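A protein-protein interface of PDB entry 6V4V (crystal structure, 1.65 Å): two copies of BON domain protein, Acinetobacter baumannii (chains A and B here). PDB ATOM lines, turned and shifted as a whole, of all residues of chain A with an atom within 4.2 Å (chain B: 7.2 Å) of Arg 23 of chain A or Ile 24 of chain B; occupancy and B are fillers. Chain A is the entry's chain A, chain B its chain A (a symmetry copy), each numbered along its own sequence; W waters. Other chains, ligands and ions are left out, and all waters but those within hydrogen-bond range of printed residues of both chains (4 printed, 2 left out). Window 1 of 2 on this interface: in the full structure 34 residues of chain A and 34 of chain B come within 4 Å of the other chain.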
ATOM      1  N   SER A  22     -14.815 -19.156 -20.675  1.00  0.00           N
ATOM      2  CA  SER A  22     -13.746 -18.516 -19.926  1.00  0.00           C
ATOM      3  C   SER A  22     -14.185 -17.200 -19.298  1.00  0.00           C
ATOM      4  O   SER A  22     -15.187 -16.588 -19.686  1.00  0.00           O
ATOM      5  CB  SER A  22     -12.547 -18.241 -20.842  1.00  0.00           C
ATOM      6  OG  SER A  22     -12.049 -19.433 -21.428  1.00  0.00           O
ATOM      7  N   ARG A  23     -13.392 -16.772 -18.312  1.00  0.00           N
ATOM      8  CA  ARG A  23     -13.396 -15.414 -17.779  1.00  0.00           C
ATOM      9  C   ARG A  23     -11.948 -14.955 -17.792  1.00  0.00           C
ATOM     10  O   ARG A  23     -11.091 -15.621 -17.207  1.00  0.00           O
ATOM     11  CB  ARG A  23     -13.964 -15.396 -16.358  1.00  0.00           C
ATOM     12  CG  ARG A  23     -13.717 -14.111 -15.566  1.00  0.00           C
ATOM     13  CD  ARG A  23     -14.526 -14.157 -14.273  1.00  0.00           C
ATOM     14  NE  ARG A  23     -14.097 -13.160 -13.302  1.00  0.00           N
ATOM     15  CZ  ARG A  23     -14.598 -11.940 -13.197  1.00  0.00           C
ATOM     16  NH1 ARG A  23     -15.549 -11.522 -14.022  1.00  0.00           N
ATOM     17  NH2 ARG A  23     -14.114 -11.115 -12.276  1.00  0.00           N
ATOM     18  N   ILE A  24     -11.645 -13.877 -18.507  1.00  0.00           N
ATOM     19  CA  ILE A  24     -10.259 -13.410 -18.612  1.00  0.00           C
ATOM     20  C   ILE A  24     -10.240 -11.929 -18.272  1.00  0.00           C
ATOM     21  O   ILE A  24     -10.791 -11.107 -19.016  1.00  0.00           O
ATOM     22  CB  ILE A  24      -9.668 -13.655 -20.005  1.00  0.00           C
ATOM     23  CG1 ILE A  24      -9.689 -15.152 -20.319  1.00  0.00           C
ATOM     24  CG2 ILE A  24      -8.234 -13.087 -20.092  1.00  0.00           C
ATOM     25  CD1 ILE A  24      -9.007 -15.490 -21.649  1.00  0.00           C
ATOM     26  N   ASN A  25      -9.645 -11.596 -17.131  1.00  0.00           N
ATOM     27  CA  ASN A  25      -9.455 -10.216 -16.702  1.00  0.00           C
ATOM     28  C   ASN A  25      -8.040  -9.771 -17.030  1.00  0.00           C
ATOM     29  O   ASN A  25      -7.083 -10.404 -16.591  1.00  0.00           O
ATOM     30  CB  ASN A  25      -9.656 -10.075 -15.197  1.00  0.00           C
ATOM     31  CG  ASN A  25     -10.947 -10.647 -14.737  1.00  0.00           C
ATOM     32  OD1 ASN A  25     -12.006 -10.308 -15.274  1.00  0.00           O
ATOM     33  ND2 ASN A  25     -10.890 -11.504 -13.724  1.00  0.00           N
ATOM     34  N   THR A  36      -6.029 -12.472 -14.493  1.00  0.00           N
ATOM     35  CA  THR A  36      -6.732 -13.387 -13.607  1.00  0.00           C
ATOM     36  C   THR A  36      -7.927 -13.953 -14.360  1.00  0.00           C
ATOM     37  O   THR A  36      -8.311 -13.446 -15.424  1.00  0.00           O
ATOM     38  CB  THR A  36      -7.217 -12.721 -12.311  1.00  0.00           C
ATOM     39  OG1 THR A  36      -8.087 -11.632 -12.631  1.00  0.00           O
ATOM     40  CG2 THR A  36      -6.057 -12.205 -11.470  1.00  0.00           C
ATOM     41  N   GLY A  37      -8.523 -15.002 -13.796  1.00  0.00           N
ATOM     42  CA  GLY A  37      -9.704 -15.576 -14.413  1.00  0.00           C
ATOM     43  C   GLY A  37      -9.577 -17.082 -14.538  1.00  0.00           C
ATOM     44  O   GLY A  37      -8.727 -17.706 -13.893  1.00  0.00           O
ATOM     45  N   GLN A  38     -10.432 -17.666 -15.384  1.00  0.00           N
ATOM     46  CA  GLN A  38     -10.562 -19.120 -15.519  1.00  0.00           C
ATOM     47  C   GLN A  38     -10.674 -19.478 -16.994  1.00  0.00           C
ATOM     48  O   GLN A  38     -11.446 -18.841 -17.717  1.00  0.00           O
ATOM     49  CB  GLN A  38     -11.816 -19.644 -14.771  1.00  0.00           C
ATOM     50  CG  GLN A  38     -11.827 -19.353 -13.280  1.00  0.00           C
ATOM     51  CD  GLN A  38     -12.408 -17.974 -12.973  1.00  0.00           C
ATOM     52  OE1 GLN A  38     -13.442 -17.593 -13.511  1.00  0.00           O
ATOM     53  NE2 GLN A  38     -11.723 -17.216 -12.120  1.00  0.00           N
ATOM     54  N   LYS A  70     -15.392 -21.503 -14.923  1.00  0.00           N
ATOM     55  CA  LYS A  70     -15.606 -20.117 -14.520  1.00  0.00           C
ATOM     56  C   LYS A  70     -16.267 -20.070 -13.147  1.00  0.00           C
ATOM     57  O   LYS A  70     -17.126 -20.897 -12.830  1.00  0.00           O
ATOM     58  CB  LYS A  70     -16.473 -19.398 -15.557  1.00  0.00           C
ATOM     59  CG  LYS A  70     -16.685 -17.914 -15.282  1.00  0.00           C
ATOM     60  CD  LYS A  70     -17.219 -17.201 -16.520  1.00  0.00           C
ATOM     61  CE  LYS A  70     -18.652 -16.773 -16.331  1.00  0.00           C
ATOM     62  NZ  LYS A  70     -19.078 -15.785 -17.358  1.00  0.00           N
ATOM     63  N   TYR A  73     -21.511 -16.184 -10.233  1.00  0.00           N
ATOM     64  CA  TYR A  73     -21.888 -14.789 -10.049  1.00  0.00           C
ATOM     65  C   TYR A  73     -21.683 -14.350  -8.605  1.00  0.00           C
ATOM     66  O   TYR A  73     -21.112 -13.285  -8.349  1.00  0.00           O
ATOM     67  CB  TYR A  73     -23.345 -14.594 -10.466  1.00  0.00           C
ATOM     68  CG  TYR A  73     -23.838 -13.176 -10.272  1.00  0.00           C
ATOM     69  CD1 TYR A  73     -23.674 -12.223 -11.274  1.00  0.00           C
ATOM     70  CD2 TYR A  73     -24.471 -12.790  -9.092  1.00  0.00           C
ATOM     71  CE1 TYR A  73     -24.140 -10.916 -11.110  1.00  0.00           C
ATOM     72  CE2 TYR A  73     -24.930 -11.488  -8.910  1.00  0.00           C
ATOM     73  CZ  TYR A  73     -24.749 -10.556  -9.919  1.00  0.00           C
ATOM     74  OH  TYR A  73     -25.202  -9.273  -9.746  1.00  0.00           O
ATOM     75  N   ILE A  76     -18.022 -13.546  -7.972  1.00  0.00           N
ATOM     76  CA  ILE A  76     -17.454 -12.274  -8.429  1.00  0.00           C
ATOM     77  C   ILE A  76     -17.991 -11.103  -7.602  1.00  0.00           C
ATOM     78  O   ILE A  76     -17.287 -10.105  -7.404  1.00  0.00           O
ATOM     79  CB  ILE A  76     -17.656 -12.044  -9.946  1.00  0.00           C
ATOM     80  CG1 ILE A  76     -19.085 -11.644 -10.301  1.00  0.00           C
ATOM     81  CG2 ILE A  76     -17.149 -13.260 -10.776  1.00  0.00           C
ATOM     82  CD1 ILE A  76     -19.160 -10.882 -11.608  1.00  0.00           C
ATOM     83  N   GLU A 106      -9.852 -12.189  -7.128  1.00  0.00           N
ATOM     84  CA  GLU A 106     -10.397 -13.217  -8.008  1.00  0.00           C
ATOM     85  C   GLU A 106     -10.484 -14.515  -7.230  1.00  0.00           C
ATOM     86  O   GLU A 106      -9.463 -15.011  -6.744  1.00  0.00           O
ATOM     87  CB  GLU A 106      -9.532 -13.395  -9.256  1.00  0.00           C
ATOM     88  CG  GLU A 106     -10.178 -14.316 -10.300  1.00  0.00           C
ATOM     89  CD  GLU A 106     -11.333 -13.651 -11.022  1.00  0.00           C
ATOM     90  OE1 GLU A 106     -11.366 -12.406 -11.086  1.00  0.00           O
ATOM     91  OE2 GLU A 106     -12.209 -14.375 -11.526  1.00  0.00           O
ATOM     92  N   ARG B  18     -27.393 -17.876 -16.863  1.00  0.00           N
ATOM     93  CA  ARG B  18     -27.278 -16.563 -17.496  1.00  0.00           C
ATOM     94  C   ARG B  18     -25.883 -15.973 -17.307  1.00  0.00           C
ATOM     95  O   ARG B  18     -25.340 -15.330 -18.222  1.00  0.00           O
ATOM     96  CB  ARG B  18     -28.356 -15.635 -16.944  1.00  0.00           C
ATOM     97  CG  ARG B  18     -29.751 -16.024 -17.398  1.00  0.00           C
ATOM     98  CD  ARG B  18     -30.767 -15.663 -16.346  1.00  0.00           C
ATOM     99  NE  ARG B  18     -30.878 -14.220 -16.151  1.00  0.00           N
ATOM    100  CZ  ARG B  18     -31.040 -13.640 -14.968  1.00  0.00           C
ATOM    101  NH1 ARG B  18     -31.110 -14.374 -13.861  1.00  0.00           N
ATOM    102  NH2 ARG B  18     -31.134 -12.322 -14.893  1.00  0.00           N
ATOM    103  N   PHE B  19     -25.290 -16.165 -16.128  1.00  0.00           N
ATOM    104  CA  PHE B  19     -23.951 -15.639 -15.906  1.00  0.00           C
ATOM    105  C   PHE B  19     -22.919 -16.398 -16.734  1.00  0.00           C
ATOM    106  O   PHE B  19     -21.906 -15.819 -17.139  1.00  0.00           O
ATOM    107  CB  PHE B  19     -23.573 -15.697 -14.425  1.00  0.00           C
ATOM    108  CG  PHE B  19     -22.220 -15.095 -14.144  1.00  0.00           C
ATOM    109  CD1 PHE B  19     -21.949 -13.784 -14.525  1.00  0.00           C
ATOM    110  CD2 PHE B  19     -21.200 -15.854 -13.588  1.00  0.00           C
ATOM    111  CE1 PHE B  19     -20.698 -13.218 -14.312  1.00  0.00           C
ATOM    112  CE2 PHE B  19     -19.935 -15.295 -13.368  1.00  0.00           C
ATOM    113  CZ  PHE B  19     -19.682 -13.983 -13.734  1.00  0.00           C
ATOM    114  N   SER B  22     -22.300 -14.545 -19.765  1.00  0.00           N
ATOM    115  CA  SER B  22     -21.991 -13.147 -19.508  1.00  0.00           C
ATOM    116  C   SER B  22     -20.495 -12.900 -19.365  1.00  0.00           C
ATOM    117  O   SER B  22     -19.697 -13.814 -19.126  1.00  0.00           O
ATOM    118  CB  SER B  22     -22.686 -12.677 -18.224  1.00  0.00           C
ATOM    119  OG  SER B  22     -24.094 -12.831 -18.302  1.00  0.00           O
ATOM    120  N   ARG B  23     -20.135 -11.622 -19.510  1.00  0.00           N
ATOM    121  CA  ARG B  23     -18.844 -11.077 -19.104  1.00  0.00           C
ATOM    122  C   ARG B  23     -19.153  -9.852 -18.261  1.00  0.00           C
ATOM    123  O   ARG B  23     -19.850  -8.948 -18.728  1.00  0.00           O
ATOM    124  CB  ARG B  23     -18.010 -10.701 -20.331  1.00  0.00           C
ATOM    125  CG  ARG B  23     -16.792  -9.818 -20.054  1.00  0.00           C
ATOM    126  CD  ARG B  23     -15.947  -9.720 -21.321  1.00  0.00           C
ATOM    127  NE  ARG B  23     -14.972  -8.640 -21.268  1.00  0.00           N
ATOM    128  CZ  ARG B  23     -13.729  -8.763 -20.831  1.00  0.00           C
ATOM    129  NH1 ARG B  23     -13.280  -9.924 -20.373  1.00  0.00           N
ATOM    130  NH2 ARG B  23     -12.935  -7.698 -20.821  1.00  0.00           N
ATOM    131  N   ILE B  24     -18.717  -9.836 -17.007  1.00  0.00           N
ATOM    132  CA  ILE B  24     -19.027  -8.712 -16.117  1.00  0.00           C
ATOM    133  C   ILE B  24     -17.725  -8.239 -15.493  1.00  0.00           C
ATOM    134  O   ILE B  24     -17.108  -8.964 -14.701  1.00  0.00           O
ATOM    135  CB  ILE B  24     -20.042  -9.094 -15.032  1.00  0.00           C
ATOM    136  CG1 ILE B  24     -21.346  -9.556 -15.685  1.00  0.00           C
ATOM    137  CG2 ILE B  24     -20.287  -7.904 -14.079  1.00  0.00           C
ATOM    138  CD1 ILE B  24     -22.451  -9.844 -14.664  1.00  0.00           C
ATOM    139  N   ASN B  25     -17.287  -7.045 -15.881  1.00  0.00           N
ATOM    140  CA  ASN B  25     -16.110  -6.402 -15.313  1.00  0.00           C
ATOM    141  C   ASN B  25     -16.538  -5.389 -14.265  1.00  0.00           C
ATOM    142  O   ASN B  25     -17.312  -4.485 -14.570  1.00  0.00           O
ATOM    143  CB  ASN B  25     -15.315  -5.664 -16.384  1.00  0.00           C
ATOM    144  CG  ASN B  25     -14.992  -6.525 -17.550  1.00  0.00           C
ATOM    145  OD1 ASN B  25     -14.444  -7.619 -17.385  1.00  0.00           O
ATOM    146  ND2 ASN B  25     -15.302  -6.042 -18.748  1.00  0.00           N
ATOM    147  N   ILE B  26     -15.987  -5.502 -13.059  1.00  0.00           N
ATOM    148  CA  ILE B  26     -16.277  -4.579 -11.964  1.00  0.00           C
ATOM    149  C   ILE B  26     -14.955  -3.944 -11.587  1.00  0.00           C
ATOM    150  O   ILE B  26     -14.069  -4.627 -11.056  1.00  0.00           O
ATOM    151  CB  ILE B  26     -16.893  -5.300 -10.756  1.00  0.00           C
ATOM    152  CG1 ILE B  26     -18.084  -6.152 -11.187  1.00  0.00           C
ATOM    153  CG2 ILE B  26     -17.262  -4.318  -9.647  1.00  0.00           C
ATOM    154  CD1 ILE B  26     -18.548  -7.119 -10.108  1.00  0.00           C
ATOM    155  N   LEU B  35     -18.877  -0.499 -14.271  1.00  0.00           N
ATOM    156  CA  LEU B  35     -19.308  -1.814 -14.742  1.00  0.00           C
ATOM    157  C   LEU B  35     -19.299  -1.811 -16.259  1.00  0.00           C
ATOM    158  O   LEU B  35     -19.891  -0.926 -16.882  1.00  0.00           O
ATOM    159  CB  LEU B  35     -20.727  -2.157 -14.270  1.00  0.00           C
ATOM    160  CG  LEU B  35     -21.034  -2.037 -12.791  1.00  0.00           C
ATOM    161  CD1 LEU B  35     -22.472  -2.490 -12.523  1.00  0.00           C
ATOM    162  CD2 LEU B  35     -20.066  -2.858 -12.005  1.00  0.00           C
ATOM    163  N   THR B  36     -18.621  -2.793 -16.854  1.00  0.00           N
ATOM    164  CA  THR B  36     -18.676  -3.000 -18.294  1.00  0.00           C
ATOM    165  C   THR B  36     -18.869  -4.487 -18.553  1.00  0.00           C
ATOM    166  O   THR B  36     -18.706  -5.319 -17.650  1.00  0.00           O
ATOM    167  CB  THR B  36     -17.414  -2.517 -19.022  1.00  0.00           C
ATOM    168  OG1 THR B  36     -16.272  -3.202 -18.503  1.00  0.00           O
ATOM    169  CG2 THR B  36     -17.210  -1.015 -18.868  1.00  0.00           C
ATOM    170  N   GLY B  37     -19.207  -4.818 -19.798  1.00  0.00           N
ATOM    171  CA  GLY B  37     -19.359  -6.216 -20.153  1.00  0.00           C
ATOM    172  C   GLY B  37     -20.665  -6.454 -20.887  1.00  0.00           C
ATOM    173  O   GLY B  37     -21.301  -5.514 -21.377  1.00  0.00           O
ATOM    174  N   GLN B  38     -21.065  -7.727 -20.958  1.00  0.00           N
ATOM    175  CA  GLN B  38     -22.216  -8.165 -21.756  1.00  0.00           C
ATOM    176  C   GLN B  38     -23.026  -9.173 -20.955  1.00  0.00           C
ATOM    177  O   GLN B  38     -22.446 -10.094 -20.371  1.00  0.00           O
ATOM    178  CB  GLN B  38     -21.758  -8.821 -23.086  1.00  0.00           C
ATOM    179  CG  GLN B  38     -20.938  -7.914 -23.986  1.00  0.00           C
ATOM    180  CD  GLN B  38     -19.452  -7.954 -23.633  1.00  0.00           C
ATOM    181  OE1 GLN B  38     -18.881  -9.021 -23.433  1.00  0.00           O
ATOM    182  NE2 GLN B  38     -18.831  -6.781 -23.534  1.00  0.00           N
ATOM    183  N   VAL B  39     -24.347  -9.010 -20.921  1.00  0.00           N
ATOM    184  CA  VAL B  39     -25.220  -9.964 -20.227  1.00  0.00           C
ATOM    185  C   VAL B  39     -26.407 -10.273 -21.136  1.00  0.00           C
ATOM    186  O   VAL B  39     -26.725  -9.493 -22.045  1.00  0.00           O
ATOM    187  CB  VAL B  39     -25.704  -9.420 -18.858  1.00  0.00           C
ATOM    188  CG1 VAL B  39     -24.528  -9.175 -17.888  1.00  0.00           C
ATOM    189  CG2 VAL B  39     -26.581  -8.171 -19.046  1.00  0.00           C
ATOM    190  N   LEU B  44     -30.260  -9.056 -15.427  1.00  0.00           N
ATOM    191  CA  LEU B  44     -28.920  -9.280 -14.896  1.00  0.00           C
ATOM    192  C   LEU B  44     -28.106  -7.992 -14.887  1.00  0.00           C
ATOM    193  O   LEU B  44     -27.311  -7.764 -13.968  1.00  0.00           O
ATOM    194  CB  LEU B  44     -28.218 -10.371 -15.705  1.00  0.00           C
ATOM    195  CG  LEU B  44     -26.842 -10.808 -15.195  1.00  0.00           C
ATOM    196  CD1 LEU B  44     -26.798 -11.030 -13.701  1.00  0.00           C
ATOM    197  CD2 LEU B  44     -26.406 -12.077 -15.923  1.00  0.00           C
ATOM    198  N   LYS B  45     -28.286  -7.145 -15.903  1.00  0.00           N
ATOM    199  CA  LYS B  45     -27.606  -5.855 -15.919  1.00  0.00           C
ATOM    200  C   LYS B  45     -27.995  -5.022 -14.704  1.00  0.00           C
ATOM    201  O   LYS B  45     -27.140  -4.389 -14.075  1.00  0.00           O
ATOM    202  CB  LYS B  45     -27.938  -5.097 -17.203  1.00  0.00           C
ATOM    203  CG  LYS B  45     -27.451  -3.642 -17.188  1.00  0.00           C
ATOM    204  CD  LYS B  45     -27.638  -2.988 -18.552  1.00  0.00           C
ATOM    205  CE  LYS B  45     -27.140  -1.557 -18.531  1.00  0.00           C
ATOM    206  NZ  LYS B  45     -27.186  -0.920 -19.875  1.00  0.00           N
ATOM    207  N   ALA B  48     -26.617  -6.626 -11.305  1.00  0.00           N
ATOM    208  CA  ALA B  48     -25.214  -6.291 -11.087  1.00  0.00           C
ATOM    209  C   ALA B  48     -25.064  -4.892 -10.503  1.00  0.00           C
ATOM    210  O   ALA B  48     -24.332  -4.692  -9.526  1.00  0.00           O
ATOM    211  CB  ALA B  48     -24.456  -6.419 -12.406  1.00  0.00           C
ATOM    212  N   VAL B  52     -23.686  -4.127  -6.689  1.00  0.00           N
ATOM    213  CA  VAL B  52     -22.495  -3.307  -6.483  1.00  0.00           C
ATOM    214  C   VAL B  52     -22.826  -2.069  -5.653  1.00  0.00           C
ATOM    215  O   VAL B  52     -22.059  -1.671  -4.763  1.00  0.00           O
ATOM    216  CB  VAL B  52     -21.875  -2.931  -7.840  1.00  0.00           C
ATOM    217  CG1 VAL B  52     -20.861  -1.827  -7.663  1.00  0.00           C
ATOM    218  CG2 VAL B  52     -21.241  -4.161  -8.501  1.00  0.00           C
ATOM    219  N   ILE B  65     -22.571  -1.919 -18.768  1.00  0.00           N
ATOM    220  CA  ILE B  65     -22.875  -3.250 -19.288  1.00  0.00           C
ATOM    221  C   ILE B  65     -23.877  -3.141 -20.434  1.00  0.00           C
ATOM    222  O   ILE B  65     -24.810  -2.320 -20.399  1.00  0.00           O
ATOM    223  CB  ILE B  65     -23.425  -4.131 -18.153  1.00  0.00           C
ATOM    224  CG1 ILE B  65     -22.338  -4.402 -17.096  1.00  0.00           C
ATOM    225  CG2 ILE B  65     -24.038  -5.416 -18.704  1.00  0.00           C
ATOM    226  CD1 ILE B  65     -22.859  -5.013 -15.812  1.00  0.00           C
ATOM    227  N   LYS B  70     -21.643 -12.080 -25.458  1.00  0.00           N
ATOM    228  CA  LYS B  70     -20.285 -11.773 -25.026  1.00  0.00           C
ATOM    229  C   LYS B  70     -19.403 -11.493 -26.238  1.00  0.00           C
ATOM    230  O   LYS B  70     -19.539 -12.139 -27.281  1.00  0.00           O
ATOM    231  CB  LYS B  70     -19.718 -12.937 -24.208  1.00  0.00           C
ATOM    232  CG  LYS B  70     -18.332 -12.685 -23.627  1.00  0.00           C
ATOM    233  CD  LYS B  70     -18.004 -13.701 -22.538  1.00  0.00           C
ATOM    234  CE  LYS B  70     -16.927 -14.656 -22.988  1.00  0.00           C
ATOM    235  NZ  LYS B  70     -16.347 -15.416 -21.849  1.00  0.00           N
ATOM    236  N   ILE B  76     -11.374  -8.738 -26.836  1.00  0.00           N
ATOM    237  CA  ILE B  76     -10.804  -8.327 -25.550  1.00  0.00           C
ATOM    238  C   ILE B  76      -9.300  -8.068 -25.671  1.00  0.00           C
ATOM    239  O   ILE B  76      -8.754  -7.217 -24.958  1.00  0.00           O
ATOM    240  CB  ILE B  76     -11.122  -9.327 -24.412  1.00  0.00           C
ATOM    241  CG1 ILE B  76     -10.283 -10.599 -24.487  1.00  0.00           C
ATOM    242  CG2 ILE B  76     -12.650  -9.620 -24.326  1.00  0.00           C
ATOM    243  CD1 ILE B  76     -10.155 -11.282 -23.142  1.00  0.00           C
ATOM    244  N   GLU B 106     -13.741  -1.512 -23.447  1.00  0.00           N
ATOM    245  CA  GLU B 106     -14.651  -2.637 -23.629  1.00  0.00           C
ATOM    246  C   GLU B 106     -15.338  -2.483 -24.972  1.00  0.00           C
ATOM    247  O   GLU B 106     -16.014  -1.477 -25.206  1.00  0.00           O
ATOM    248  CB  GLU B 106     -15.682  -2.705 -22.502  1.00  0.00           C
ATOM    249  CG  GLU B 106     -16.525  -3.986 -22.545  1.00  0.00           C
ATOM    250  CD  GLU B 106     -15.746  -5.206 -22.096  1.00  0.00           C
ATOM    251  OE1 GLU B 106     -14.765  -5.050 -21.342  1.00  0.00           O
ATOM    252  OE2 GLU B 106     -16.114  -6.323 -22.501  1.00  0.00           O
HETATM  253  O   HOH W   1     -17.339 -12.866 -16.315  1.00  0.00           O
HETATM  254  O   HOH W   2     -16.515 -13.830 -18.730  1.00  0.00           O
HETATM  255  O   HOH W   3     -14.211 -10.423 -17.050  1.00  0.00           O
HETATM  256  O   HOH W   4     -14.421 -12.915 -20.218  1.00  0.00           O
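O of Ser 22 of chain A sits at hydrogen-bond distance from NZ of Lys 70 of chain B, at 2.7 Å. NH1 of Arg 23 of chain A is in hydrogen-bond range of O of Ile 24 of chain B, 3.1 Å away. NH1 of Arg 23 of chain B is in hydrogen-bond range of O of Ile 24 of chain A, at 3.1 Å. The backbone carbonyl oxygen of Phe 19 of chain B lies within hydrogen-bond range of the side-chain amino group of Lys 70 of chain A. NZ of Lys 70 of chain A is in hydrogen-bond range of O of Ser 22 of chain B, 2.7 Å away. N of Ala 48 of chain B sits close to OH of Tyr 73 of chain A (3.4 Å).
The backbone NH of Gln 38 of chain A sits at hydrogen-bond distance from the backbone carbonyl oxygen of Arg 23 of chain A (2.8 Å). OE2 of Glu 106 of chain A lies within salt-bridge range of NE of Arg 23 of chain A (2.9 Å). The backbone carbonyl oxygen of Arg 18 of chain B is in hydrogen-bond range of the side-chain hydroxyl of Ser 22 of chain B, 2.8 Å away. The backbone carbonyl oxygen of Arg 23 of chain B is in hydrogen-bond range of the backbone NH of Gln 38 of chain B (2.8 Å). The guanidinium group (NE) of Arg 23 of chain B lies within salt-bridge range of the side-chain carboxylate (OE2) of Glu 106 of chain B, 2.9 Å away.
CD1 of Ile 76 of chain B touches CB of Ile 24 of chain A, 3.96 Å away. Phe 19 of chain B touches Tyr 73 of chain A. CE1 of Tyr 73 of chain A touches CD1 of Leu 44 of chain B (3.7 Å). Ile 76 of chain A touches Phe 19 of chain B (CD1 to CZ, 3.8 Å). Ile 24 of chain B touches Ile 76 of chain A (CB to CD1, 3.96 Å).
Arg 23 of chain A touches just one residue of chain B: Ile 24. Of the printed residues of chain B, Ile 76 of chain A touches Phe 19 (3.8 Å) and Ile 24 (3.96 Å). Ile 24 of chain B touches just these residues of chain A: Arg 23 and Ile 76. Of the printed residues of chain A, Leu 44 of chain B touches Tyr 73 (3.7 Å). The nearest printed residue of chain B that does not touch Arg 23 of chain A is Lys 70 of chain B (4.8 Å). The nearest residue of chain A that does not touch Ile 24 of chain B is Tyr 73 of chain A (4.1 Å).
Of the 20 printed residues of chain B, 8 touch a printed residue of chain A. Hydrophobic or aromatic side chains of chain B that line the printed part of chain A: Phe 19, Ile 24, Leu 44, Ala 48 and Ile 76.
Ser 22 of chain A touches Lys 70 of chain B, and with the chains exchanged Lys 70 of chain A touches Ser 22 of chain B. Arg 23 of chain A touches Ile 24 of chain B, and with the chains exchanged Ile 24 of chain A touches Arg 23 of chain B. Ile 24 of chain A touches Ile 76 of chain B, and with the chains exchanged Ile 76 of chain A touches Ile 24 of chain B. 10 positions are printed for both chains. Of the 11 pairs that touch across the chains among the printed residues, 6 have their exchanged pair printed and touching as well.
Water W3 lies within hydrogen-bond range of OD1 of Asn 25 of chain A, OD1 of Asn 25 of chain B, NH1 of Arg 23 of chain B and NH1 of Arg 23 of chain A. Water W1 bridges the guanidinium group of Arg 23 of chain A (3.2 Å) and the backbone NH of Ile 24 of chain B (3.4 Å). Water W4 bridges NH1 of Arg 23 of chain B and N of Ile 24 of chain A. Water W2 lies within hydrogen-bond range of O of Ser 22 of chain A (3.2 Å) and O of Ser 22 of chain B (3.2 Å).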
